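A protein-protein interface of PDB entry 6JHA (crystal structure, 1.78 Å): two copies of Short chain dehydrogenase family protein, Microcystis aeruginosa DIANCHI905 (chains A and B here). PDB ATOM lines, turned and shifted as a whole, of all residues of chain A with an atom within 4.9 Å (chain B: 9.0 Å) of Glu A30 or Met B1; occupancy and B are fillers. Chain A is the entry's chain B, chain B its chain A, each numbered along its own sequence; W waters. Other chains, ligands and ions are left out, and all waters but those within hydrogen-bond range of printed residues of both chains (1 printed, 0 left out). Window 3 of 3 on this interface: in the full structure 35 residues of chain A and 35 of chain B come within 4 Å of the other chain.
Water W1 lies within hydrogen-bond range of the side-chain carboxylate of Glu B30 (2.8 Å) and the backbone NH of Met A1 (3.5 Å).
The backbone carbonyl oxygen of Met B1 is in hydrogen-bond range of the backbone NH of Met A1 (2.8 Å).
OE1 of Glu A30 lies within hydrogen-bond range of N of Met B1 (2.8 Å).
The side-chain carboxylate (OE1) of Glu B30 sits at hydrogen-bond distance from the backbone NH (N) of Met A1 (2.8 Å).
The backbone carbonyl oxygen of Cys B246 lies within hydrogen-bond range of the side-chain amide nitrogen of Asn A237.
Glu A30 touches one residue of chain B.
No residue of chain B comes within 4 Å of Gly A31.
Printed residues of chain B within 4 Å of Asn A237: Met B1 (3.8 Å), Phe B241 (3.7 Å) and Cys B246 (3.2 Å).
Of the printed residues of chain A, Met B1 touches Met A1, Leu A3, Glu A30, Asn A237 and Val A240.
Printed residues of chain A within 4 Å of Glu B30: Met A1.
Printed residues of chain A within 4 Å of Asn B237: Met A1 (3.8 Å) and Phe A241 (3.7 Å).
Of the printed residues of chain A, Val B240 touches Met A1.
The nearest printed residue of chain A that does not touch Met B1 is Phe A241 (4.7 Å).
The nearest printed residue of chain B that does not touch Val A240 is Phe B241 (6.6 Å).
Among the printed residues, 13 pairs touch across the chains.
The side-chain sulfur (SG) of Cys B246 is in hydrogen-bond range of the backbone carbonyl oxygen (O) of Asp B2 (3.3 Å).
N of Glu B245 lies within hydrogen-bond range of O of Leu B3, at 2.9 Å.
The backbone carbonyl oxygen (O) of Phe B241 lies within hydrogen-bond range of the side-chain hydroxyl (OG) of Ser B244 (2.7 Å).
N of Cys B246 sits at hydrogen-bond distance from OG of Ser B244, at 3.0 Å.
OD1 of Asn A237 sits at hydrogen-bond distance from NZ of Lys A26.
Among the printed residues, pairs that only touch across the chains: Asn A237 with Phe B241 (3.7 Å), Phe A241 with Asn B237 (3.7 Å), Val A240 with Met B1 (3.7 Å), Asn A237 with Met B1 (3.8 Å), Met A1 with Asn B237 (3.8 Å), Met A1 with Val B240 (3.9 Å), Phe A241 with Phe B241 (3.9 Å), Met A1 with Leu B3 (3.96 Å) and Leu A3 with Met B1 (3.99 Å).
Met A1 touches Leu B3, and with the chains exchanged Leu A3 touches Met B1.
Met A1 touches Glu B30, and with the chains exchanged Glu A30 touches Met B1.
Met A1 touches Asn B237, and with the chains exchanged Asn A237 touches Met B1.
Phe B241 touches its own counterpart, Phe A241.
Positions printed for both chains: 1, 3, 5, 29, 30, 237, 240 and 241.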
ATOM      1  N   MET A   1      33.018  -5.829 -26.210  1.00  0.00           N
ATOM      2  CA  MET A   1      31.930  -6.234 -25.268  1.00  0.00           C
ATOM      3  C   MET A   1      30.795  -6.933 -26.041  1.00  0.00           C
ATOM      4  O   MET A   1      30.201  -6.347 -26.966  1.00  0.00           O
ATOM      5  CB  MET A   1      31.389  -5.020 -24.525  1.00  0.00           C
ATOM      6  CG  MET A   1      30.325  -5.376 -23.491  1.00  0.00           C
ATOM      7  SD  MET A   1      29.791  -3.927 -22.515  1.00  0.00           S
ATOM      8  CE  MET A   1      31.149  -3.898 -21.339  1.00  0.00           C
ATOM      9  N   LEU A   3      27.236  -7.767 -26.521  1.00  0.00           N
ATOM     10  CA  LEU A   3      26.010  -7.114 -26.080  1.00  0.00           C
ATOM     11  C   LEU A   3      24.801  -8.043 -26.135  1.00  0.00           C
ATOM     12  O   LEU A   3      23.722  -7.632 -25.724  1.00  0.00           O
ATOM     13  CB  LEU A   3      25.751  -5.896 -26.944  1.00  0.00           C
ATOM     14  CG  LEU A   3      26.717  -4.708 -26.822  1.00  0.00           C
ATOM     15  CD1 LEU A   3      26.119  -3.551 -27.590  1.00  0.00           C
ATOM     16  CD2 LEU A   3      27.009  -4.264 -25.397  1.00  0.00           C
ATOM     17  N   LEU A   5      22.977  -9.256 -28.507  1.00  0.00           N
ATOM     18  CA  LEU A   5      21.895  -8.782 -29.384  1.00  0.00           C
ATOM     19  C   LEU A   5      21.689  -9.634 -30.631  1.00  0.00           C
ATOM     20  O   LEU A   5      20.827  -9.319 -31.471  1.00  0.00           O
ATOM     21  CB  LEU A   5      22.170  -7.342 -29.852  1.00  0.00           C
ATOM     22  CG  LEU A   5      22.064  -6.325 -28.724  1.00  0.00           C
ATOM     23  CD1 LEU A   5      22.468  -4.979 -29.288  1.00  0.00           C
ATOM     24  CD2 LEU A   5      20.618  -6.316 -28.209  1.00  0.00           C
ATOM     25  N   LYS A   6      22.488 -10.674 -30.792  1.00  0.00           N
ATOM     26  CA  LYS A   6      22.351 -11.492 -32.029  1.00  0.00           C
ATOM     27  C   LYS A   6      20.911 -12.024 -32.167  1.00  0.00           C
ATOM     28  O   LYS A   6      20.370 -12.631 -31.239  1.00  0.00           O
ATOM     29  CB  LYS A   6      23.315 -12.666 -32.012  1.00  0.00           C
ATOM     30  CG  LYS A   6      23.318 -13.507 -33.291  1.00  0.00           C
ATOM     31  CD  LYS A   6      24.575 -14.376 -33.327  1.00  0.00           C
ATOM     32  CE  LYS A   6      24.852 -14.901 -34.730  1.00  0.00           C
ATOM     33  NZ  LYS A   6      23.698 -15.707 -35.201  1.00  0.00           N
ATOM     34  N   LYS A  26      24.057   0.613 -36.196  1.00  0.00           N
ATOM     35  CA  LYS A  26      24.782   0.059 -35.094  1.00  0.00           C
ATOM     36  C   LYS A  26      24.085  -1.184 -34.488  1.00  0.00           C
ATOM     37  O   LYS A  26      24.752  -2.123 -34.060  1.00  0.00           O
ATOM     38  CB  LYS A  26      25.023   1.095 -34.006  1.00  0.00           C
ATOM     39  CG  LYS A  26      26.003   2.188 -34.398  1.00  0.00           C
ATOM     40  CD  LYS A  26      27.328   2.005 -33.661  1.00  0.00           C
ATOM     41  CE  LYS A  26      28.359   2.991 -34.147  1.00  0.00           C
ATOM     42  NZ  LYS A  26      29.647   2.794 -33.443  1.00  0.00           N
ATOM     43  N   LEU A  27      22.759  -1.195 -34.473  1.00  0.00           N
ATOM     44  CA  LEU A  27      22.060  -2.372 -34.050  1.00  0.00           C
ATOM     45  C   LEU A  27      22.255  -3.537 -35.039  1.00  0.00           C
ATOM     46  O   LEU A  27      22.414  -4.670 -34.608  1.00  0.00           O
ATOM     47  CB  LEU A  27      20.557  -2.086 -33.850  1.00  0.00           C
ATOM     48  CG  LEU A  27      20.190  -1.265 -32.601  1.00  0.00           C
ATOM     49  CD1 LEU A  27      18.766  -0.718 -32.693  1.00  0.00           C
ATOM     50  CD2 LEU A  27      20.397  -2.004 -31.276  1.00  0.00           C
ATOM     51  N   ALA A  28      22.236  -3.246 -36.347  1.00  0.00           N
ATOM     52  CA  ALA A  28      22.538  -4.270 -37.372  1.00  0.00           C
ATOM     53  C   ALA A  28      23.966  -4.829 -37.175  1.00  0.00           C
ATOM     54  O   ALA A  28      24.205  -6.052 -37.270  1.00  0.00           O
ATOM     55  CB  ALA A  28      22.363  -3.682 -38.745  1.00  0.00           C
ATOM     56  N   GLU A  29      24.905  -3.960 -36.851  1.00  0.00           N
ATOM     57  CA  GLU A  29      26.288  -4.369 -36.610  1.00  0.00           C
ATOM     58  C   GLU A  29      26.400  -5.347 -35.466  1.00  0.00           C
ATOM     59  O   GLU A  29      27.247  -6.244 -35.508  1.00  0.00           O
ATOM     60  CB  GLU A  29      27.160  -3.157 -36.316  1.00  0.00           C
ATOM     61  CG  GLU A  29      28.654  -3.480 -36.195  1.00  0.00           C
ATOM     62  CD  GLU A  29      29.446  -3.083 -37.425  1.00  0.00           C
ATOM     63  OE1 GLU A  29      30.285  -3.898 -37.888  1.00  0.00           O
ATOM     64  OE2 GLU A  29      29.239  -1.946 -37.934  1.00  0.00           O
ATOM     65  N   GLU A  30      25.534  -5.224 -34.463  1.00  0.00           N
ATOM     66  CA  GLU A  30      25.590  -6.080 -33.296  1.00  0.00           C
ATOM     67  C   GLU A  30      24.749  -7.356 -33.498  1.00  0.00           C
ATOM     68  O   GLU A  30      24.619  -8.181 -32.602  1.00  0.00           O
ATOM     69  CB  GLU A  30      25.158  -5.336 -32.031  1.00  0.00           C
ATOM     70  CG  GLU A  30      25.973  -4.092 -31.692  1.00  0.00           C
ATOM     71  CD  GLU A  30      27.434  -4.367 -31.415  1.00  0.00           C
ATOM     72  OE1 GLU A  30      27.703  -5.176 -30.533  1.00  0.00           O
ATOM     73  OE2 GLU A  30      28.303  -3.812 -32.121  1.00  0.00           O
ATOM     74  N   GLY A  31      24.142  -7.488 -34.665  1.00  0.00           N
ATOM     75  CA  GLY A  31      23.455  -8.728 -35.026  1.00  0.00           C
ATOM     76  C   GLY A  31      21.944  -8.700 -34.971  1.00  0.00           C
ATOM     77  O   GLY A  31      21.313  -9.743 -35.131  1.00  0.00           O
ATOM     78  N   CYS A  32      21.341  -7.526 -34.832  1.00  0.00           N
ATOM     79  CA  CYS A  32      19.878  -7.425 -34.824  1.00  0.00           C
ATOM     80  C   CYS A  32      19.307  -7.482 -36.202  1.00  0.00           C
ATOM     81  O   CYS A  32      19.914  -7.020 -37.165  1.00  0.00           O
ATOM     82  CB  CYS A  32      19.358  -6.096 -34.249  1.00  0.00           C
ATOM     83  SG  CYS A  32      19.792  -5.763 -32.537  1.00  0.00           S
ATOM     84  N   ASN A 237      26.033   4.868 -29.815  1.00  0.00           N
ATOM     85  CA  ASN A 237      26.681   3.898 -28.930  1.00  0.00           C
ATOM     86  C   ASN A 237      25.936   3.672 -27.646  1.00  0.00           C
ATOM     87  O   ASN A 237      25.828   2.554 -27.164  1.00  0.00           O
ATOM     88  CB  ASN A 237      28.121   4.296 -28.604  1.00  0.00           C
ATOM     89  CG  ASN A 237      29.048   4.131 -29.779  1.00  0.00           C
ATOM     90  OD1 ASN A 237      28.802   3.310 -30.663  1.00  0.00           O
ATOM     91  ND2 ASN A 237      30.120   4.919 -29.804  1.00  0.00           N
ATOM     92  N   VAL A 240      22.534   1.852 -28.202  1.00  0.00           N
ATOM     93  CA  VAL A 240      22.748   0.430 -28.445  1.00  0.00           C
ATOM     94  C   VAL A 240      23.122  -0.317 -27.151  1.00  0.00           C
ATOM     95  O   VAL A 240      22.626  -1.412 -26.874  1.00  0.00           O
ATOM     96  CB  VAL A 240      23.773   0.247 -29.591  1.00  0.00           C
ATOM     97  CG1 VAL A 240      24.165  -1.215 -29.715  1.00  0.00           C
ATOM     98  CG2 VAL A 240      23.115   0.720 -30.873  1.00  0.00           C
ATOM     99  N   PHE A 241      23.918   0.318 -26.292  1.00  0.00           N
ATOM    100  CA  PHE A 241      24.204  -0.240 -24.975  1.00  0.00           C
ATOM    101  C   PHE A 241      22.962  -0.445 -24.112  1.00  0.00           C
ATOM    102  O   PHE A 241      22.764  -1.526 -23.486  1.00  0.00           O
ATOM    103  CB  PHE A 241      25.215   0.611 -24.186  1.00  0.00           C
ATOM    104  CG  PHE A 241      25.533   0.019 -22.854  1.00  0.00           C
ATOM    105  CD1 PHE A 241      26.458  -1.001 -22.736  1.00  0.00           C
ATOM    106  CD2 PHE A 241      24.879   0.464 -21.715  1.00  0.00           C
ATOM    107  CE1 PHE A 241      26.744  -1.537 -21.502  1.00  0.00           C
ATOM    108  CE2 PHE A 241      25.146  -0.084 -20.480  1.00  0.00           C
ATOM    109  CZ  PHE A 241      26.055  -1.117 -20.372  1.00  0.00           C
ATOM    110  N   MET B   1      30.320  -5.006 -29.476  1.00  0.00           N
ATOM    111  CA  MET B   1      30.709  -3.581 -29.617  1.00  0.00           C
ATOM    112  C   MET B   1      32.168  -3.409 -29.247  1.00  0.00           C
ATOM    113  O   MET B   1      32.580  -3.832 -28.172  1.00  0.00           O
ATOM    114  CB  MET B   1      29.834  -2.682 -28.749  1.00  0.00           C
ATOM    115  CG  MET B   1      30.183  -1.205 -28.829  1.00  0.00           C
ATOM    116  SD  MET B   1      29.064  -0.175 -27.851  1.00  0.00           S
ATOM    117  CE  MET B   1      27.686  -0.161 -28.994  1.00  0.00           C
ATOM    118  N   ASP B   2      32.932  -2.825 -30.166  1.00  0.00           N
ATOM    119  CA  ASP B   2      34.342  -2.556 -29.944  1.00  0.00           C
ATOM    120  C   ASP B   2      34.506  -1.287 -29.117  1.00  0.00           C
ATOM    121  O   ASP B   2      34.258  -0.153 -29.607  1.00  0.00           O
ATOM    122  CB  ASP B   2      35.084  -2.323 -31.282  1.00  0.00           C
ATOM    123  CG  ASP B   2      36.613  -2.121 -31.107  1.00  0.00           C
ATOM    124  OD1 ASP B   2      37.140  -1.988 -29.980  1.00  0.00           O
ATOM    125  OD2 ASP B   2      37.324  -2.078 -32.154  1.00  0.00           O
ATOM    126  N   LEU B   3      34.946  -1.470 -27.894  1.00  0.00           N
ATOM    127  CA  LEU B   3      35.108  -0.358 -26.911  1.00  0.00           C
ATOM    128  C   LEU B   3      36.389   0.485 -26.999  1.00  0.00           C
ATOM    129  O   LEU B   3      36.556   1.474 -26.290  1.00  0.00           O
ATOM    130  CB  LEU B   3      34.933  -0.929 -25.501  1.00  0.00           C
ATOM    131  CG  LEU B   3      33.558  -1.510 -25.173  1.00  0.00           C
ATOM    132  CD1 LEU B   3      33.474  -1.697 -23.671  1.00  0.00           C
ATOM    133  CD2 LEU B   3      32.465  -0.555 -25.571  1.00  0.00           C
ATOM    134  N   GLY B   4      37.312   0.099 -27.871  1.00  0.00           N
ATOM    135  CA  GLY B   4      38.508   0.871 -28.083  1.00  0.00           C
ATOM    136  C   GLY B   4      39.469   0.903 -26.893  1.00  0.00           C
ATOM    137  O   GLY B   4      40.207   1.862 -26.734  1.00  0.00           O
ATOM    138  N   LEU B   5      39.527  -0.178 -26.132  1.00  0.00           N
ATOM    139  CA  LEU B   5      40.244  -0.179 -24.857  1.00  0.00           C
ATOM    140  C   LEU B   5      41.513  -1.013 -24.892  1.00  0.00           C
ATOM    141  O   LEU B   5      42.235  -1.135 -23.880  1.00  0.00           O
ATOM    142  CB  LEU B   5      39.351  -0.727 -23.735  1.00  0.00           C
ATOM    143  CG  LEU B   5      38.283   0.228 -23.294  1.00  0.00           C
ATOM    144  CD1 LEU B   5      37.329  -0.467 -22.361  1.00  0.00           C
ATOM    145  CD2 LEU B   5      38.892   1.478 -22.687  1.00  0.00           C
ATOM    146  N   GLU B  29      39.019  -8.034 -19.809  1.00  0.00           N
ATOM    147  CA  GLU B  29      38.355  -8.712 -20.914  1.00  0.00           C
ATOM    148  C   GLU B  29      38.318  -7.847 -22.172  1.00  0.00           C
ATOM    149  O   GLU B  29      38.465  -8.362 -23.286  1.00  0.00           O
ATOM    150  CB  GLU B  29      36.947  -9.178 -20.504  1.00  0.00           C
ATOM    151  CG  GLU B  29      36.492 -10.362 -21.350  1.00  0.00           C
ATOM    152  CD  GLU B  29      35.092 -10.856 -21.015  1.00  0.00           C
ATOM    153  OE1 GLU B  29      34.414 -10.285 -20.121  1.00  0.00           O
ATOM    154  OE2 GLU B  29      34.669 -11.825 -21.688  1.00  0.00           O
ATOM    155  N   GLU B  30      38.209  -6.522 -22.004  1.00  0.00           N
ATOM    156  CA  GLU B  30      38.226  -5.610 -23.128  1.00  0.00           C
ATOM    157  C   GLU B  30      39.638  -5.226 -23.563  1.00  0.00           C
ATOM    158  O   GLU B  30      39.808  -4.433 -24.514  1.00  0.00           O
ATOM    159  CB  GLU B  30      37.430  -4.333 -22.808  1.00  0.00           C
ATOM    160  CG  GLU B  30      35.941  -4.552 -22.513  1.00  0.00           C
ATOM    161  CD  GLU B  30      35.194  -5.286 -23.605  1.00  0.00           C
ATOM    162  OE1 GLU B  30      35.145  -4.802 -24.777  1.00  0.00           O
ATOM    163  OE2 GLU B  30      34.672  -6.371 -23.280  1.00  0.00           O
ATOM    164  N   ASN B 237      29.302  -3.668 -16.253  1.00  0.00           N
ATOM    165  CA  ASN B 237      29.103  -3.402 -17.669  1.00  0.00           C
ATOM    166  C   ASN B 237      28.962  -1.916 -18.006  1.00  0.00           C
ATOM    167  O   ASN B 237      29.511  -1.413 -19.011  1.00  0.00           O
ATOM    168  CB  ASN B 237      27.885  -4.152 -18.212  1.00  0.00           C
ATOM    169  CG  ASN B 237      28.137  -5.625 -18.411  1.00  0.00           C
ATOM    170  OD1 ASN B 237      29.273  -6.066 -18.607  1.00  0.00           O
ATOM    171  ND2 ASN B 237      27.058  -6.398 -18.366  1.00  0.00           N
ATOM    172  N   VAL B 240      32.379  -0.029 -17.476  1.00  0.00           N
ATOM    173  CA  VAL B 240      33.281  -0.283 -18.599  1.00  0.00           C
ATOM    174  C   VAL B 240      32.831   0.489 -19.826  1.00  0.00           C
ATOM    175  O   VAL B 240      33.674   1.041 -20.550  1.00  0.00           O
ATOM    176  CB  VAL B 240      33.390  -1.763 -18.885  1.00  0.00           C
ATOM    177  CG1 VAL B 240      34.291  -2.011 -20.101  1.00  0.00           C
ATOM    178  CG2 VAL B 240      34.042  -2.443 -17.696  1.00  0.00           C
ATOM    179  N   PHE B 241      31.531   0.575 -20.066  1.00  0.00           N
ATOM    180  CA  PHE B 241      31.063   1.455 -21.165  1.00  0.00           C
ATOM    181  C   PHE B 241      31.523   2.891 -20.979  1.00  0.00           C
ATOM    182  O   PHE B 241      32.050   3.526 -21.917  1.00  0.00           O
ATOM    183  CB  PHE B 241      29.548   1.359 -21.361  1.00  0.00           C
ATOM    184  CG  PHE B 241      29.046   2.203 -22.491  1.00  0.00           C
ATOM    185  CD1 PHE B 241      29.093   1.732 -23.774  1.00  0.00           C
ATOM    186  CD2 PHE B 241      28.559   3.479 -22.252  1.00  0.00           C
ATOM    187  CE1 PHE B 241      28.644   2.537 -24.830  1.00  0.00           C
ATOM    188  CE2 PHE B 241      28.145   4.282 -23.279  1.00  0.00           C
ATOM    189  CZ  PHE B 241      28.159   3.799 -24.567  1.00  0.00           C
ATOM    190  N   SER B 244      35.102   3.742 -21.886  1.00  0.00           N
ATOM    191  CA  SER B 244      35.475   3.337 -23.243  1.00  0.00           C
ATOM    192  C   SER B 244      35.582   4.520 -24.238  1.00  0.00           C
ATOM    193  O   SER B 244      35.119   5.608 -23.997  1.00  0.00           O
ATOM    194  CB  SER B 244      34.469   2.350 -23.813  1.00  0.00           C
ATOM    195  OG  SER B 244      33.291   3.002 -24.269  1.00  0.00           O
ATOM    196  N   GLU B 245      36.140   4.242 -25.402  1.00  0.00           N
ATOM    197  CA  GLU B 245      36.131   5.218 -26.473  1.00  0.00           C
ATOM    198  C   GLU B 245      34.697   5.526 -26.907  1.00  0.00           C
ATOM    199  O   GLU B 245      34.404   6.649 -27.355  1.00  0.00           O
ATOM    200  CB  GLU B 245      36.894   4.654 -27.685  1.00  0.00           C
ATOM    201  CG  GLU B 245      37.160   5.717 -28.730  1.00  0.00           C
ATOM    202  CD  GLU B 245      38.190   6.750 -28.331  1.00  0.00           C
ATOM    203  OE1 GLU B 245      38.990   6.472 -27.441  1.00  0.00           O
ATOM    204  OE2 GLU B 245      38.250   7.821 -29.002  1.00  0.00           O
ATOM    205  N   CYS B 246      33.781   4.559 -26.730  1.00  0.00           N
ATOM    206  CA  CYS B 246      32.397   4.719 -27.189  1.00  0.00           C
ATOM    207  C   CYS B 246      31.616   5.773 -26.409  1.00  0.00           C
ATOM    208  O   CYS B 246      30.605   6.271 -26.926  1.00  0.00           O
ATOM    209  CB  CYS B 246      31.643   3.378 -27.092  1.00  0.00           C
ATOM    210  SG  CYS B 246      32.284   2.162 -28.232  1.00  0.00           S
ATOM    211  N   ALA B 247      32.081   6.111 -25.205  1.00  0.00           N
ATOM    212  CA  ALA B 247      31.466   7.123 -24.368  1.00  0.00           C
ATOM    213  C   ALA B 247      32.115   8.517 -24.555  1.00  0.00           C
ATOM    214  O   ALA B 247      32.066   9.367 -23.664  1.00  0.00           O
ATOM    215  CB  ALA B 247      31.529   6.674 -22.923  1.00  0.00           C
HETATM  216  O   HOH W   1      34.994  -8.446 -25.064  1.00  0.00           O
